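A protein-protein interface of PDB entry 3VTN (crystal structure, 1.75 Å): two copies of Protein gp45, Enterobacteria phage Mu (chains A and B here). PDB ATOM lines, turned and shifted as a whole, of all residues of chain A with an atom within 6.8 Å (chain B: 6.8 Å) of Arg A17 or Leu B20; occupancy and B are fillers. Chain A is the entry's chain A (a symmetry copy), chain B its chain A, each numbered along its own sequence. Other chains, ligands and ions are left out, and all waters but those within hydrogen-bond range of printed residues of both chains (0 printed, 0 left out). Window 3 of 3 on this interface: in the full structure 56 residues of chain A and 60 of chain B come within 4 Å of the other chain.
Of the 10 printed residues of chain B, 4 touch a printed residue of chain A.
Of the 8 printed residues of chain A, 4 touch a printed residue of chain B.
Hydrophobic or aromatic side chains of chain A that line the printed part of chain B: Ile A18 and Ile A28.
Among the printed residues, 5 pairs touch across the chains.
Among the printed residues, no Asp or Glu carboxylate lies within 4 Å of a Lys or Arg side-chain nitrogen of the other chain.
The backbone carbonyl oxygen (O) of Arg A17 is in hydrogen-bond range of the backbone NH (N) of Thr A29, 2.9 Å away.
Arg A17 touches Leu B20, but with the chains exchanged Leu A20 does not touch Arg B17 (13.3 Å).
Ile A18 touches its own counterpart, Ile B18.
Of the 5 pairs that touch across the chains among the printed residues, 1 has its exchanged pair printed and touching as well.
Of chain B, only Leu B20 comes within 4 Å of Arg A17.
Of the printed residues of chain B, Cys A30 touches Gly B24 and Cys B26.
Of the printed residues of chain B, Ile A18 touches Ile B18 (3.7 Å).
Printed residues of chain A within 4 Å of Ile B18: Ile A18.
The nearest residue of chain A that does not touch Leu B20 is Ile A18 (4.2 Å).
The nearest printed residue of chain B that does not touch Ile A28 is Leu B20 (6.6 Å).
Leu B20 touches Arg A17 (CD2 to N, 3.5 Å).
Ile A18 touches Ile B18.
Ile A28 touches Cys B26 (CG2 to SG, 3.8 Å).
Cys A30 touches Gly B24 (CB to O, 3.5 Å).
Cys A30 touches Cys B26.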
ATOM      1  N   ARG A  17     -17.183 -17.447  -3.383  1.00  0.00           N
ATOM      2  CA  ARG A  17     -17.345 -15.965  -3.518  1.00  0.00           C
ATOM      3  C   ARG A  17     -16.310 -15.324  -4.456  1.00  0.00           C
ATOM      4  O   ARG A  17     -15.106 -15.354  -4.192  1.00  0.00           O
ATOM      5  CB  ARG A  17     -17.318 -15.305  -2.143  1.00  0.00           C
ATOM      6  CG  ARG A  17     -17.259 -13.787  -2.196  1.00  0.00           C
ATOM      7  CD  ARG A  17     -17.967 -13.137  -1.010  1.00  0.00           C
ATOM      8  NE  ARG A  17     -18.228 -11.719  -1.276  1.00  0.00           N
ATOM      9  CZ  ARG A  17     -19.145 -11.261  -2.137  1.00  0.00           C
ATOM     10  NH1 ARG A  17     -19.913 -12.099  -2.838  1.00  0.00           N
ATOM     11  NH2 ARG A  17     -19.295  -9.948  -2.304  1.00  0.00           N
ATOM     12  N   ILE A  18     -16.798 -14.754  -5.551  1.00  0.00           N
ATOM     13  CA  ILE A  18     -15.963 -14.049  -6.503  1.00  0.00           C
ATOM     14  C   ILE A  18     -16.392 -12.589  -6.486  1.00  0.00           C
ATOM     15  O   ILE A  18     -17.529 -12.268  -6.864  1.00  0.00           O
ATOM     16  CB  ILE A  18     -16.066 -14.660  -7.936  1.00  0.00           C
ATOM     17  CG1 ILE A  18     -15.564 -16.112  -7.936  1.00  0.00           C
ATOM     18  CG2 ILE A  18     -15.320 -13.800  -8.963  1.00  0.00           C
ATOM     19  CD1 ILE A  18     -15.566 -16.806  -9.297  1.00  0.00           C
ATOM     20  N   ARG A  19     -15.497 -11.711  -6.021  1.00  0.00           N
ATOM     21  CA  ARG A  19     -15.739 -10.260  -6.038  1.00  0.00           C
ATOM     22  C   ARG A  19     -14.984  -9.551  -7.157  1.00  0.00           C
ATOM     23  O   ARG A  19     -13.782  -9.753  -7.340  1.00  0.00           O
ATOM     24  CB  ARG A  19     -15.347  -9.610  -4.709  1.00  0.00           C
ATOM     25  CG  ARG A  19     -15.939 -10.242  -3.481  1.00  0.00           C
ATOM     26  CD  ARG A  19     -15.779  -9.326  -2.290  1.00  0.00           C
ATOM     27  NE  ARG A  19     -16.158  -7.957  -2.644  1.00  0.00           N
ATOM     28  CZ  ARG A  19     -16.493  -7.015  -1.768  1.00  0.00           C
ATOM     29  NH1 ARG A  19     -16.516  -7.292  -0.460  1.00  0.00           N
ATOM     30  NH2 ARG A  19     -16.820  -5.803  -2.206  1.00  0.00           N
ATOM     31  N   LEU A  20     -15.705  -8.704  -7.886  1.00  0.00           N
ATOM     32  CA  LEU A  20     -15.136  -7.790  -8.861  1.00  0.00           C
ATOM     33  C   LEU A  20     -15.179  -6.383  -8.278  1.00  0.00           C
ATOM     34  O   LEU A  20     -16.148  -5.996  -7.622  1.00  0.00           O
ATOM     35  CB  LEU A  20     -15.924  -7.858 -10.164  1.00  0.00           C
ATOM     36  CG  LEU A  20     -15.452  -8.931 -11.146  1.00  0.00           C
ATOM     37  CD1 LEU A  20     -15.383 -10.296 -10.525  1.00  0.00           C
ATOM     38  CD2 LEU A  20     -16.392  -8.948 -12.339  1.00  0.00           C
ATOM     39  N   ILE A  27     -11.204 -10.820  -6.829  1.00  0.00           N
ATOM     40  CA  ILE A  27     -10.944 -11.584  -5.606  1.00  0.00           C
ATOM     41  C   ILE A  27     -11.784 -12.846  -5.605  1.00  0.00           C
ATOM     42  O   ILE A  27     -13.003 -12.776  -5.675  1.00  0.00           O
ATOM     43  CB  ILE A  27     -11.247 -10.752  -4.350  1.00  0.00           C
ATOM     44  CG1 ILE A  27     -10.621  -9.375  -4.515  1.00  0.00           C
ATOM     45  CG2 ILE A  27     -10.765 -11.473  -3.061  1.00  0.00           C
ATOM     46  CD1 ILE A  27     -11.153  -8.284  -3.584  1.00  0.00           C
ATOM     47  N   ILE A  28     -11.116 -13.994  -5.549  1.00  0.00           N
ATOM     48  CA  ILE A  28     -11.798 -15.288  -5.414  1.00  0.00           C
ATOM     49  C   ILE A  28     -11.429 -15.848  -4.052  1.00  0.00           C
ATOM     50  O   ILE A  28     -10.241 -16.123  -3.782  1.00  0.00           O
ATOM     51  CB  ILE A  28     -11.361 -16.313  -6.483  1.00  0.00           C
ATOM     52  CG1 ILE A  28     -11.637 -15.816  -7.906  1.00  0.00           C
ATOM     53  CG2 ILE A  28     -12.045 -17.650  -6.205  1.00  0.00           C
ATOM     54  CD1 ILE A  28     -10.671 -16.388  -8.967  1.00  0.00           C
ATOM     55  N   THR A  29     -12.428 -16.009  -3.176  1.00  0.00           N
ATOM     56  CA  THR A  29     -12.221 -16.507  -1.808  1.00  0.00           C
ATOM     57  C   THR A  29     -13.004 -17.795  -1.505  1.00  0.00           C
ATOM     58  O   THR A  29     -14.235 -17.773  -1.412  1.00  0.00           O
ATOM     59  CB  THR A  29     -12.559 -15.433  -0.731  1.00  0.00           C
ATOM     60  OG1 THR A  29     -12.062 -14.166  -1.148  1.00  0.00           O
ATOM     61  CG2 THR A  29     -11.905 -15.772   0.605  1.00  0.00           C
ATOM     62  N   CYS A  30     -12.301 -18.913  -1.360  1.00  0.00           N
ATOM     63  CA  CYS A  30     -12.945 -20.186  -0.989  1.00  0.00           C
ATOM     64  C   CYS A  30     -11.990 -21.162  -0.306  1.00  0.00           C
ATOM     65  O   CYS A  30     -10.890 -20.787   0.066  1.00  0.00           O
ATOM     66  CB  CYS A  30     -13.478 -20.837  -2.232  1.00  0.00           C
ATOM     67  SG  CYS A  30     -12.189 -20.921  -3.361  1.00  0.00           S
ATOM     68  N   ARG B  17     -17.933 -22.284 -17.586  1.00  0.00           N
ATOM     69  CA  ARG B  17     -18.697 -22.681 -16.362  1.00  0.00           C
ATOM     70  C   ARG B  17     -17.898 -22.504 -15.062  1.00  0.00           C
ATOM     71  O   ARG B  17     -16.869 -23.152 -14.854  1.00  0.00           O
ATOM     72  CB  ARG B  17     -19.205 -24.113 -16.502  1.00  0.00           C
ATOM     73  CG  ARG B  17     -19.806 -24.674 -15.222  1.00  0.00           C
ATOM     74  CD  ARG B  17     -20.923 -25.677 -15.497  1.00  0.00           C
ATOM     75  NE  ARG B  17     -21.725 -25.903 -14.291  1.00  0.00           N
ATOM     76  CZ  ARG B  17     -22.581 -25.017 -13.767  1.00  0.00           C
ATOM     77  NH1 ARG B  17     -22.769 -23.822 -14.333  1.00  0.00           N
ATOM     78  NH2 ARG B  17     -23.257 -25.328 -12.661  1.00  0.00           N
ATOM     79  N   ILE B  18     -18.384 -21.618 -14.201  1.00  0.00           N
ATOM     80  CA  ILE B  18     -17.786 -21.382 -12.902  1.00  0.00           C
ATOM     81  C   ILE B  18     -18.803 -21.804 -11.853  1.00  0.00           C
ATOM     82  O   ILE B  18     -19.880 -21.197 -11.748  1.00  0.00           O
ATOM     83  CB  ILE B  18     -17.357 -19.892 -12.718  1.00  0.00           C
ATOM     84  CG1 ILE B  18     -16.281 -19.515 -13.748  1.00  0.00           C
ATOM     85  CG2 ILE B  18     -16.891 -19.620 -11.282  1.00  0.00           C
ATOM     86  CD1 ILE B  18     -15.740 -18.090 -13.636  1.00  0.00           C
ATOM     87  N   ARG B  19     -18.479 -22.860 -11.100  1.00  0.00           N
ATOM     88  CA  ARG B  19     -19.322 -23.317  -9.984  1.00  0.00           C
ATOM     89  C   ARG B  19     -18.767 -22.913  -8.623  1.00  0.00           C
ATOM     90  O   ARG B  19     -17.586 -23.112  -8.333  1.00  0.00           O
ATOM     91  CB  ARG B  19     -19.495 -24.838  -9.998  1.00  0.00           C
ATOM     92  CG  ARG B  19     -19.959 -25.425 -11.302  1.00  0.00           C
ATOM     93  CD  ARG B  19     -20.428 -26.847 -11.100  1.00  0.00           C
ATOM     94  NE  ARG B  19     -21.296 -26.936  -9.926  1.00  0.00           N
ATOM     95  CZ  ARG B  19     -22.158 -27.923  -9.696  1.00  0.00           C
ATOM     96  NH1 ARG B  19     -22.288 -28.919 -10.578  1.00  0.00           N
ATOM     97  NH2 ARG B  19     -22.897 -27.901  -8.591  1.00  0.00           N
ATOM     98  N   LEU B  20     -19.643 -22.360  -7.790  1.00  0.00           N
ATOM     99  CA  LEU B  20     -19.367 -22.089  -6.389  1.00  0.00           C
ATOM    100  C   LEU B  20     -20.122 -23.110  -5.548  1.00  0.00           C
ATOM    101  O   LEU B  20     -21.262 -23.467  -5.853  1.00  0.00           O
ATOM    102  CB  LEU B  20     -19.803 -20.672  -6.035  1.00  0.00           C
ATOM    103  CG  LEU B  20     -18.745 -19.594  -6.277  1.00  0.00           C
ATOM    104  CD1 LEU B  20     -18.199 -19.620  -7.675  1.00  0.00           C
ATOM    105  CD2 LEU B  20     -19.356 -18.235  -5.982  1.00  0.00           C
ATOM    106  N   THR B  21     -19.484 -23.584  -4.493  1.00  0.00           N
ATOM    107  CA  THR B  21     -19.933 -24.772  -3.822  1.00  0.00           C
ATOM    108  C   THR B  21     -20.069 -24.551  -2.298  1.00  0.00           C
ATOM    109  O   THR B  21     -19.183 -24.015  -1.632  1.00  0.00           O
ATOM    110  CB  THR B  21     -18.963 -25.908  -4.203  1.00  0.00           C
ATOM    111  OG1 THR B  21     -19.404 -26.557  -5.413  1.00  0.00           O
ATOM    112  CG2 THR B  21     -18.789 -26.865  -3.153  1.00  0.00           C
ATOM    113  N   LYS B  22     -21.216 -24.933  -1.757  1.00  0.00           N
ATOM    114  CA  LYS B  22     -21.340 -25.081  -0.322  1.00  0.00           C
ATOM    115  C   LYS B  22     -20.331 -26.198  -0.061  1.00  0.00           C
ATOM    116  O   LYS B  22     -20.153 -27.081  -0.895  1.00  0.00           O
ATOM    117  CB  LYS B  22     -22.774 -25.507   0.022  1.00  0.00           C
ATOM    118  CG  LYS B  22     -23.835 -24.682  -0.693  1.00  0.00           C
ATOM    119  CD  LYS B  22     -24.285 -23.539   0.194  1.00  0.00           C
ATOM    120  CE  LYS B  22     -24.717 -22.307  -0.607  1.00  0.00           C
ATOM    121  NZ  LYS B  22     -24.863 -21.106   0.305  1.00  0.00           N
ATOM    122  N   GLY B  24     -17.323 -25.395   0.042  1.00  0.00           N
ATOM    123  CA  GLY B  24     -16.208 -24.458  -0.185  1.00  0.00           C
ATOM    124  C   GLY B  24     -15.309 -24.673  -1.407  1.00  0.00           C
ATOM    125  O   GLY B  24     -14.172 -24.204  -1.400  1.00  0.00           O
ATOM    126  N   ARG B  25     -15.807 -25.361  -2.438  1.00  0.00           N
ATOM    127  CA  ARG B  25     -15.066 -25.533  -3.716  1.00  0.00           C
ATOM    128  C   ARG B  25     -15.465 -24.436  -4.729  1.00  0.00           C
ATOM    129  O   ARG B  25     -16.634 -24.090  -4.878  1.00  0.00           O
ATOM    130  CB  ARG B  25     -15.347 -26.900  -4.331  1.00  0.00           C
ATOM    131  CG  ARG B  25     -14.901 -28.042  -3.457  1.00  0.00           C
ATOM    132  CD  ARG B  25     -15.349 -29.401  -3.975  1.00  0.00           C
ATOM    133  NE  ARG B  25     -16.780 -29.570  -3.726  1.00  0.00           N
ATOM    134  CZ  ARG B  25     -17.714 -29.966  -4.589  1.00  0.00           C
ATOM    135  NH1 ARG B  25     -17.423 -30.351  -5.838  1.00  0.00           N
ATOM    136  NH2 ARG B  25     -18.964 -30.015  -4.161  1.00  0.00           N
ATOM    137  N   CYS B  26     -14.466 -23.855  -5.393  1.00  0.00           N
ATOM    138  CA  CYS B  26     -14.657 -22.970  -6.532  1.00  0.00           C
ATOM    139  C   CYS B  26     -14.073 -23.670  -7.753  1.00  0.00           C
ATOM    140  O   CYS B  26     -12.851 -23.879  -7.819  1.00  0.00           O
ATOM    141  CB  CYS B  26     -13.915 -21.646  -6.295  1.00  0.00           C
ATOM    142  SG  CYS B  26     -13.801 -20.601  -7.781  1.00  0.00           S
ATOM    143  N   ILE B  27     -14.936 -24.065  -8.676  1.00  0.00           N
ATOM    144  CA  ILE B  27     -14.590 -24.903  -9.827  1.00  0.00           C
ATOM    145  C   ILE B  27     -14.781 -24.115 -11.107  1.00  0.00           C
ATOM    146  O   ILE B  27     -15.875 -23.643 -11.385  1.00  0.00           O
ATOM    147  CB  ILE B  27     -15.442 -26.181  -9.866  1.00  0.00           C
ATOM    148  CG1 ILE B  27     -15.461 -26.798  -8.475  1.00  0.00           C
ATOM    149  CG2 ILE B  27     -14.931 -27.173 -10.948  1.00  0.00           C
ATOM    150  CD1 ILE B  27     -16.570 -27.817  -8.211  1.00  0.00           C
